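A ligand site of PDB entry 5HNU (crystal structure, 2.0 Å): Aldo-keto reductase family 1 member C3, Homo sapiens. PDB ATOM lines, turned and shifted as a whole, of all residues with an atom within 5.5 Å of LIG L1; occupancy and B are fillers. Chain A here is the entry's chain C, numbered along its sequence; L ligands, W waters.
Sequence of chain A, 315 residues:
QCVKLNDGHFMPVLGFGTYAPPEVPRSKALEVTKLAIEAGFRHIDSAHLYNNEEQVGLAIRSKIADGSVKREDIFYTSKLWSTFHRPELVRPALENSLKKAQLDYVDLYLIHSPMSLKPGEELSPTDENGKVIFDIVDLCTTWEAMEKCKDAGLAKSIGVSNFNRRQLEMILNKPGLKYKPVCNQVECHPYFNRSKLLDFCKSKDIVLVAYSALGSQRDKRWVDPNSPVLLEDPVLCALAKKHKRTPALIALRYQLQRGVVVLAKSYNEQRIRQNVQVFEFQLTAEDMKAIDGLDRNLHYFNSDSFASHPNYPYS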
ATOM      1  N   TYR A  19      -3.517   7.599 -20.088  1.00  0.00           N
ATOM      2  CA  TYR A  19      -2.100   7.773 -19.717  1.00  0.00           C
ATOM      3  C   TYR A  19      -1.198   8.033 -20.944  1.00  0.00           C
ATOM      4  O   TYR A  19      -1.299   7.318 -21.918  1.00  0.00           O
ATOM      5  CB  TYR A  19      -1.484   6.557 -18.976  1.00  0.00           C
ATOM      6  CG  TYR A  19      -0.004   6.821 -18.600  1.00  0.00           C
ATOM      7  CD1 TYR A  19       0.315   7.612 -17.505  1.00  0.00           C
ATOM      8  CD2 TYR A  19       1.036   6.359 -19.411  1.00  0.00           C
ATOM      9  CE1 TYR A  19       1.623   7.880 -17.162  1.00  0.00           C
ATOM     10  CE2 TYR A  19       2.356   6.618 -19.085  1.00  0.00           C
ATOM     11  CZ  TYR A  19       2.644   7.406 -17.968  1.00  0.00           C
ATOM     12  OH  TYR A  19       3.942   7.704 -17.636  1.00  0.00           O
ATOM     13  N   LEU A  49      -1.928   8.931 -10.429  1.00  0.00           N
ATOM     14  CA  LEU A  49      -0.634   8.704 -11.023  1.00  0.00           C
ATOM     15  C   LEU A  49      -0.385   9.411 -12.347  1.00  0.00           C
ATOM     16  O   LEU A  49       0.730   9.799 -12.613  1.00  0.00           O
ATOM     17  CB  LEU A  49      -0.365   7.197 -11.216  1.00  0.00           C
ATOM     18  CG  LEU A  49       0.993   6.774 -11.789  1.00  0.00           C
ATOM     19  CD1 LEU A  49       2.168   7.121 -10.868  1.00  0.00           C
ATOM     20  CD2 LEU A  49       0.953   5.300 -12.067  1.00  0.00           C
ATOM     21  N   TYR A  50      -1.417   9.618 -13.148  1.00  0.00           N
ATOM     22  CA  TYR A  50      -1.197  10.008 -14.550  1.00  0.00           C
ATOM     23  C   TYR A  50      -0.906  11.472 -14.738  1.00  0.00           C
ATOM     24  O   TYR A  50      -0.587  11.864 -15.872  1.00  0.00           O
ATOM     25  CB  TYR A  50      -2.411   9.616 -15.412  1.00  0.00           C
ATOM     26  CG  TYR A  50      -2.769   8.107 -15.372  1.00  0.00           C
ATOM     27  CD1 TYR A  50      -1.896   7.148 -14.846  1.00  0.00           C
ATOM     28  CD2 TYR A  50      -3.953   7.644 -15.956  1.00  0.00           C
ATOM     29  CE1 TYR A  50      -2.226   5.787 -14.818  1.00  0.00           C
ATOM     30  CE2 TYR A  50      -4.249   6.272 -15.975  1.00  0.00           C
ATOM     31  CZ  TYR A  50      -3.390   5.371 -15.399  1.00  0.00           C
ATOM     32  OH  TYR A  50      -3.689   4.026 -15.379  1.00  0.00           O
ATOM     33  N   LYS A  79      -8.072   6.474  -9.660  1.00  0.00           N
ATOM     34  CA  LYS A  79      -7.392   5.456  -8.900  1.00  0.00           C
ATOM     35  C   LYS A  79      -6.586   6.074  -7.751  1.00  0.00           C
ATOM     36  O   LYS A  79      -5.979   7.131  -7.915  1.00  0.00           O
ATOM     37  CB  LYS A  79      -6.485   4.553  -9.778  1.00  0.00           C
ATOM     38  CG  LYS A  79      -7.090   4.132 -11.123  1.00  0.00           C
ATOM     39  CD  LYS A  79      -6.203   3.116 -11.843  1.00  0.00           C
ATOM     40  CE  LYS A  79      -6.693   2.834 -13.244  1.00  0.00           C
ATOM     41  NZ  LYS A  79      -6.356   3.850 -14.262  1.00  0.00           N
ATOM     42  N   TRP A  81      -3.580   6.151  -5.458  1.00  0.00           N
ATOM     43  CA  TRP A  81      -2.219   5.809  -5.623  1.00  0.00           C
ATOM     44  C   TRP A  81      -1.712   5.169  -4.338  1.00  0.00           C
ATOM     45  O   TRP A  81      -2.235   5.363  -3.243  1.00  0.00           O
ATOM     46  CB  TRP A  81      -1.401   7.041  -6.110  1.00  0.00           C
ATOM     47  CG  TRP A  81       0.047   6.711  -6.349  1.00  0.00           C
ATOM     48  CD1 TRP A  81       1.132   7.300  -5.713  1.00  0.00           C
ATOM     49  CD2 TRP A  81       0.578   5.708  -7.195  1.00  0.00           C
ATOM     50  NE1 TRP A  81       2.286   6.681  -6.099  1.00  0.00           N
ATOM     51  CE2 TRP A  81       1.989   5.690  -6.994  1.00  0.00           C
ATOM     52  CE3 TRP A  81       0.012   4.751  -8.048  1.00  0.00           C
ATOM     53  CZ2 TRP A  81       2.832   4.811  -7.647  1.00  0.00           C
ATOM     54  CZ3 TRP A  81       0.883   3.842  -8.707  1.00  0.00           C
ATOM     55  CH2 TRP A  81       2.261   3.881  -8.493  1.00  0.00           C
ATOM     56  N   HIS A 112      -5.091   1.277  -7.013  1.00  0.00           N
ATOM     57  CA  HIS A 112      -4.278   1.201  -8.256  1.00  0.00           C
ATOM     58  C   HIS A 112      -3.364  -0.052  -8.286  1.00  0.00           C
ATOM     59  O   HIS A 112      -3.195  -0.670  -9.318  1.00  0.00           O
ATOM     60  CB  HIS A 112      -3.439   2.476  -8.405  1.00  0.00           C
ATOM     61  CG  HIS A 112      -3.069   2.791  -9.824  1.00  0.00           C
ATOM     62  ND1 HIS A 112      -2.874   4.072 -10.265  1.00  0.00           N
ATOM     63  CD2 HIS A 112      -2.816   1.987 -10.883  1.00  0.00           C
ATOM     64  CE1 HIS A 112      -2.534   4.053 -11.538  1.00  0.00           C
ATOM     65  NE2 HIS A 112      -2.506   2.793 -11.936  1.00  0.00           N
ATOM     66  N   VAL A 132      12.484   4.941  -3.656  1.00  0.00           N
ATOM     67  CA  VAL A 132      11.329   3.976  -3.584  1.00  0.00           C
ATOM     68  C   VAL A 132      11.262   3.270  -2.263  1.00  0.00           C
ATOM     69  O   VAL A 132      12.041   2.352  -1.998  1.00  0.00           O
ATOM     70  CB  VAL A 132      11.167   2.892  -4.680  1.00  0.00           C
ATOM     71  CG1 VAL A 132       9.746   2.326  -4.676  1.00  0.00           C
ATOM     72  CG2 VAL A 132      11.451   3.504  -6.015  1.00  0.00           C
ATOM     73  N   ASN A 162      -4.459  -4.610 -10.560  1.00  0.00           N
ATOM     74  CA  ASN A 162      -3.197  -5.356 -10.393  1.00  0.00           C
ATOM     75  C   ASN A 162      -3.182  -6.323  -9.234  1.00  0.00           C
ATOM     76  O   ASN A 162      -2.101  -6.643  -8.725  1.00  0.00           O
ATOM     77  CB  ASN A 162      -1.966  -4.413 -10.312  1.00  0.00           C
ATOM     78  CG  ASN A 162      -1.777  -3.630 -11.597  1.00  0.00           C
ATOM     79  OD1 ASN A 162      -1.571  -4.213 -12.679  1.00  0.00           O
ATOM     80  ND2 ASN A 162      -1.925  -2.277 -11.504  1.00  0.00           N
ATOM     81  N   GLN A 185      -8.785  -4.429 -12.602  1.00  0.00           N
ATOM     82  CA  GLN A 185      -8.152  -3.909 -13.825  1.00  0.00           C
ATOM     83  C   GLN A 185      -6.726  -4.421 -13.844  1.00  0.00           C
ATOM     84  O   GLN A 185      -5.926  -4.034 -12.992  1.00  0.00           O
ATOM     85  CB  GLN A 185      -8.178  -2.366 -13.867  1.00  0.00           C
ATOM     86  CG  GLN A 185      -7.524  -1.802 -15.132  1.00  0.00           C
ATOM     87  CD  GLN A 185      -7.522  -0.289 -15.234  1.00  0.00           C
ATOM     88  OE1 GLN A 185      -6.458   0.312 -15.469  1.00  0.00           O
ATOM     89  NE2 GLN A 185      -8.676   0.336 -15.085  1.00  0.00           N
ATOM     90  N   ASP A 219       6.925   1.671 -23.643  1.00  0.00           N
ATOM     91  CA  ASP A 219       7.691   2.764 -23.086  1.00  0.00           C
ATOM     92  C   ASP A 219       9.129   2.253 -22.804  1.00  0.00           C
ATOM     93  O   ASP A 219       9.360   1.300 -22.060  1.00  0.00           O
ATOM     94  CB  ASP A 219       7.024   3.236 -21.791  1.00  0.00           C
ATOM     95  CG  ASP A 219       7.581   4.560 -21.280  1.00  0.00           C
ATOM     96  OD1 ASP A 219       8.825   4.672 -21.141  1.00  0.00           O
ATOM     97  OD2 ASP A 219       6.770   5.490 -20.987  1.00  0.00           O
ATOM     98  N   ARG A 221      11.449   3.324 -21.001  1.00  0.00           N
ATOM     99  CA  ARG A 221      11.797   3.281 -19.605  1.00  0.00           C
ATOM    100  C   ARG A 221      11.644   1.870 -18.990  1.00  0.00           C
ATOM    101  O   ARG A 221      12.355   1.566 -18.024  1.00  0.00           O
ATOM    102  CB  ARG A 221      10.972   4.320 -18.794  1.00  0.00           C
ATOM    103  CG  ARG A 221      11.228   5.815 -19.115  1.00  0.00           C
ATOM    104  CD  ARG A 221      10.252   6.747 -18.357  1.00  0.00           C
ATOM    105  NE  ARG A 221       8.841   6.521 -18.751  1.00  0.00           N
ATOM    106  CZ  ARG A 221       7.741   6.817 -18.019  1.00  0.00           C
ATOM    107  NH1 ARG A 221       6.510   6.531 -18.493  1.00  0.00           N
ATOM    108  NH2 ARG A 221       7.833   7.378 -16.813  1.00  0.00           N
ATOM    109  N   TRP A 222      10.702   1.049 -19.478  1.00  0.00           N
ATOM    110  CA  TRP A 222      10.486  -0.322 -18.907  1.00  0.00           C
ATOM    111  C   TRP A 222      10.614  -1.390 -19.944  1.00  0.00           C
ATOM    112  O   TRP A 222      11.354  -2.345 -19.759  1.00  0.00           O
ATOM    113  CB  TRP A 222       9.081  -0.558 -18.283  1.00  0.00           C
ATOM    114  CG  TRP A 222       8.534   0.671 -17.840  1.00  0.00           C
ATOM    115  CD1 TRP A 222       7.474   1.334 -18.371  1.00  0.00           C
ATOM    116  CD2 TRP A 222       9.080   1.526 -16.816  1.00  0.00           C
ATOM    117  NE1 TRP A 222       7.315   2.531 -17.741  1.00  0.00           N
ATOM    118  CE2 TRP A 222       8.274   2.674 -16.772  1.00  0.00           C
ATOM    119  CE3 TRP A 222      10.180   1.408 -15.922  1.00  0.00           C
ATOM    120  CZ2 TRP A 222       8.519   3.734 -15.864  1.00  0.00           C
ATOM    121  CZ3 TRP A 222      10.428   2.467 -15.006  1.00  0.00           C
ATOM    122  CH2 TRP A 222       9.597   3.606 -14.998  1.00  0.00           C
ATOM    123  N   PHE A 301       4.368  -4.958 -18.570  1.00  0.00           N
ATOM    124  CA  PHE A 301       4.745  -4.284 -17.337  1.00  0.00           C
ATOM    125  C   PHE A 301       5.796  -5.188 -16.636  1.00  0.00           C
ATOM    126  O   PHE A 301       5.452  -6.112 -15.879  1.00  0.00           O
ATOM    127  CB  PHE A 301       3.487  -3.824 -16.565  1.00  0.00           C
ATOM    128  CG  PHE A 301       2.886  -2.567 -17.204  1.00  0.00           C
ATOM    129  CD1 PHE A 301       2.401  -2.635 -18.518  1.00  0.00           C
ATOM    130  CD2 PHE A 301       2.951  -1.314 -16.591  1.00  0.00           C
ATOM    131  CE1 PHE A 301       1.956  -1.517 -19.181  1.00  0.00           C
ATOM    132  CE2 PHE A 301       2.469  -0.172 -17.257  1.00  0.00           C
ATOM    133  CZ  PHE A 301       1.998  -0.273 -18.550  1.00  0.00           C
ATOM    134  N   SER A 305      11.741  -4.387 -11.037  1.00  0.00           N
ATOM    135  CA  SER A 305      12.122  -3.400 -10.000  1.00  0.00           C
ATOM    136  C   SER A 305      11.491  -3.676  -8.606  1.00  0.00           C
ATOM    137  O   SER A 305      12.175  -3.686  -7.567  1.00  0.00           O
ATOM    138  CB  SER A 305      11.614  -2.046 -10.556  1.00  0.00           C
ATOM    139  OG  SER A 305      11.780  -0.947  -9.676  1.00  0.00           O
ATOM    140  N   PHE A 306      10.194  -3.966  -8.643  1.00  0.00           N
ATOM    141  CA  PHE A 306       9.319  -4.114  -7.457  1.00  0.00           C
ATOM    142  C   PHE A 306       9.162  -5.538  -6.984  1.00  0.00           C
ATOM    143  O   PHE A 306       8.388  -5.819  -6.039  1.00  0.00           O
ATOM    144  CB  PHE A 306       7.938  -3.509  -7.750  1.00  0.00           C
ATOM    145  CG  PHE A 306       7.946  -2.011  -7.771  1.00  0.00           C
ATOM    146  CD1 PHE A 306       8.688  -1.352  -8.733  1.00  0.00           C
ATOM    147  CD2 PHE A 306       7.280  -1.250  -6.796  1.00  0.00           C
ATOM    148  CE1 PHE A 306       8.772   0.025  -8.753  1.00  0.00           C
ATOM    149  CE2 PHE A 306       7.348   0.149  -6.827  1.00  0.00           C
ATOM    150  CZ  PHE A 306       8.104   0.786  -7.810  1.00  0.00           C
HETATM  151  O1  LIG L   1      -1.869   2.673 -14.559  1.00  0.00           O
HETATM  152  C1  LIG L   1       6.137   4.194 -11.912  1.00  0.00           C
HETATM  153  C2  LIG L   1       5.281   3.144 -12.623  1.00  0.00           C
HETATM  154  O2  LIG L   1      -1.351   3.476 -17.213  1.00  0.00           O
HETATM  155  C3  LIG L   1       5.885   2.487 -13.879  1.00  0.00           C
HETATM  156  C4  LIG L   1       4.977   2.387 -15.108  1.00  0.00           C
HETATM  157  C5  LIG L   1       3.346   3.788 -16.183  1.00  0.00           C
HETATM  158  C6  LIG L   1       1.986   3.289 -15.817  1.00  0.00           C
HETATM  159  C7  LIG L   1       0.939   3.564 -16.686  1.00  0.00           C
HETATM  160  C8  LIG L   1      -0.357   3.261 -16.323  1.00  0.00           C
HETATM  161  C9  LIG L   1      -0.626   2.695 -15.093  1.00  0.00           C
HETATM  162  C10 LIG L   1       0.434   2.302 -14.276  1.00  0.00           C
HETATM  163  C11 LIG L   1       1.738   2.600 -14.642  1.00  0.00           C
HETATM  164  O3  LIG L   1       3.657   4.223 -17.261  1.00  0.00           O
HETATM  165  O4  LIG L   1       0.152   1.647 -13.136  1.00  0.00           O
HETATM  166  O5  LIG L   1       4.214   3.621 -15.192  1.00  0.00           O
HETATM  167  C12 LIG L   1       7.236   3.623 -11.017  1.00  0.00           C
HETATM  168  C13 LIG L   1       8.597   3.349 -11.700  1.00  0.00           C
HETATM  169  C14 LIG L   1       9.589   2.403 -10.933  1.00  0.00           C
HETATM  170  C15 LIG L   1      11.108   2.614 -11.126  1.00  0.00           C
HETATM  171  P1  LG2 L   2      -2.872   0.302 -25.038  1.00  0.00           P
HETATM  172  O1  LG2 L   2      -4.310   0.609 -24.928  1.00  0.00           O
HETATM  173  O2  LG2 L   2      -2.326  -1.108 -25.172  1.00  0.00           O
HETATM  174  O3  LG2 L   2      -2.320   1.014 -26.386  1.00  0.00           O
HETATM  175  C1  LG2 L   2      -0.948   0.921 -26.752  1.00  0.00           C
HETATM  176  C2  LG2 L   2      -0.760   1.705 -28.037  1.00  0.00           C
HETATM  177  O4  LG2 L   2      -1.635   1.314 -29.057  1.00  0.00           O
HETATM  178  C3  LG2 L   2      -1.103   3.188 -27.832  1.00  0.00           C
HETATM  179  O5  LG2 L   2       0.034   3.811 -27.317  1.00  0.00           O
HETATM  180  C4  LG2 L   2      -1.610   3.719 -29.152  1.00  0.00           C
HETATM  181  O6  LG2 L   2      -0.767   4.654 -29.842  1.00  0.00           O
HETATM  182  C5  LG2 L   2      -1.796   2.432 -29.956  1.00  0.00           C
HETATM  183  N1  LG2 L   2      -3.104   2.322 -30.603  1.00  0.00           N
HETATM  184  C6  LG2 L   2      -4.329   2.670 -30.106  1.00  0.00           C
HETATM  185  N2  LG2 L   2      -5.324   2.409 -30.967  1.00  0.00           N
HETATM  186  C7  LG2 L   2      -4.711   1.812 -32.051  1.00  0.00           C
HETATM  187  C8  LG2 L   2      -5.166   1.260 -33.316  1.00  0.00           C
HETATM  188  N3  LG2 L   2      -6.471   1.268 -33.526  1.00  0.00           N
HETATM  189  N4  LG2 L   2      -4.259   0.727 -34.191  1.00  0.00           N
HETATM  190  C9  LG2 L   2      -2.931   0.706 -33.895  1.00  0.00           C
HETATM  191  N5  LG2 L   2      -2.426   1.199 -32.737  1.00  0.00           N
HETATM  192  C10 LG2 L   2      -3.254   1.777 -31.816  1.00  0.00           C
HETATM  193  O7  LG2 L   2      -2.058   1.188 -23.966  1.00  0.00           O
HETATM  194  P2  LG2 L   2      -1.837   1.209 -22.368  1.00  0.00           P
HETATM  195  O8  LG2 L   2      -1.703   2.707 -22.066  1.00  0.00           O
HETATM  196  O9  LG2 L   2      -0.694   0.270 -22.079  1.00  0.00           O
HETATM  197  O10 LG2 L   2      -3.230   0.822 -21.727  1.00  0.00           O
HETATM  198  C11 LG2 L   2      -4.378   1.635 -21.964  1.00  0.00           C
HETATM  199  C12 LG2 L   2      -4.800   2.329 -20.659  1.00  0.00           C
HETATM  200  O11 LG2 L   2      -4.949   1.371 -19.578  1.00  0.00           O
HETATM  201  C13 LG2 L   2      -3.855   3.378 -20.079  1.00  0.00           C
HETATM  202  O12 LG2 L   2      -3.812   4.569 -20.853  1.00  0.00           O
HETATM  203  C14 LG2 L   2      -4.453   3.534 -18.670  1.00  0.00           C
HETATM  204  O13 LG2 L   2      -5.694   4.257 -18.719  1.00  0.00           O
HETATM  205  C15 LG2 L   2      -4.703   2.058 -18.337  1.00  0.00           C
HETATM  206  N6  LG2 L   2      -3.581   1.359 -17.663  1.00  0.00           N
HETATM  207  C16 LG2 L   2      -3.735   1.007 -16.386  1.00  0.00           C
HETATM  208  C17 LG2 L   2      -2.756   0.305 -15.681  1.00  0.00           C
HETATM  209  C18 LG2 L   2      -2.934  -0.051 -14.244  1.00  0.00           C
HETATM  210  O14 LG2 L   2      -1.966  -0.277 -13.466  1.00  0.00           O
HETATM  211  N7  LG2 L   2      -4.154  -0.138 -13.809  1.00  0.00           N
HETATM  212  C19 LG2 L   2      -1.585   0.013 -16.331  1.00  0.00           C
HETATM  213  C20 LG2 L   2      -1.449   0.340 -17.661  1.00  0.00           C
HETATM  214  C21 LG2 L   2      -2.463   0.993 -18.320  1.00  0.00           C
HETATM  215  P3  LG2 L   2      -1.239   6.157 -30.217  1.00  0.00           P
HETATM  216  O15 LG2 L   2      -0.119   6.573 -31.045  1.00  0.00           O
HETATM  217  O16 LG2 L   2      -2.467   5.870 -31.040  1.00  0.00           O
HETATM  218  O17 LG2 L   2      -1.410   6.820 -28.891  1.00  0.00           O
HETATM  219  O   HOH W   1      -0.220   3.111 -19.626  1.00  0.00           O
HETATM  220  O   HOH W   2       2.452   3.338 -20.113  1.00  0.00           O
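An oxygen (O1) of LIG L1 is in hydrogen-bond range of the side-chain hydroxyl (OH) of Tyr 50 (2.4 Å). NE2 of His 112 lies within hydrogen-bond range of O1 of LIG L1. A nitrogen (N7) of LG2 L2 is in hydrogen-bond range of the side-chain amide oxygen (OE1) of Gln 185 (2.9 Å). The side-chain amide nitrogen of Asn 162 sits at hydrogen-bond distance from an oxygen (O14) of LG2 L2 (2.8 Å). A ring nitrogen (NE2) of His 112 sits at hydrogen-bond distance from an oxygen (O14) of LG2 L2 (3.5 Å). N of Tyr 19 is in hydrogen-bond range of O12 of LG2 L2 (3.1 Å).
O4 of LIG L1 is in hydrogen-bond range of O14 of LG2 L2, at 2.9 Å.
The side-chain amino group (NZ) of Lys 79 lies within hydrogen-bond range of the side-chain hydroxyl (OH) of Tyr 50, at 2.9 Å. The backbone carbonyl oxygen (O) of His 112 sits at hydrogen-bond distance from the side-chain amide nitrogen (ND2) of Asn 162, at 3.0 Å. The guanidinium group (NH1) of Arg 221 is in salt-bridge range of the side-chain carboxylate (OD2) of Asp 219 (2.7 Å). OH of Tyr 19 sits at hydrogen-bond distance from NH1 of Arg 221, 3.0 Å away.
Tyr 19 touches LIG L1 (CE2 to O3, 3.3 Å). Leu 49 touches LIG L1. Arg 221 touches LIG L1. Trp 222 touches LIG L1 (CH2 to C13, 3.5 Å). Phe 301 touches LIG L1. OG of Ser 305 touches C15 of LIG L1, 3.9 Å away. CE1 of Phe 306 touches C14 of LIG L1, 3.3 Å away. Hydrophobic or aromatic side chains that line LIG L1: Tyr 19, Leu 49, Tyr 50, His 112, Trp 222, Phe 301 and Phe 306. Within 4 Å of LIG L1: Tyr 19, Leu 49, Tyr 50, His 112, Arg 221, Trp 222, Phe 301, Ser 305 and Phe 306. The nearest printed residue that does not touch LIG L1 is Lys 79 (4.6 Å).
Water W1 lies within hydrogen-bond range of an oxygen (O2) of LIG L1 (2.7 Å) and an oxygen (O8) of LG2 L2 (2.9 Å).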
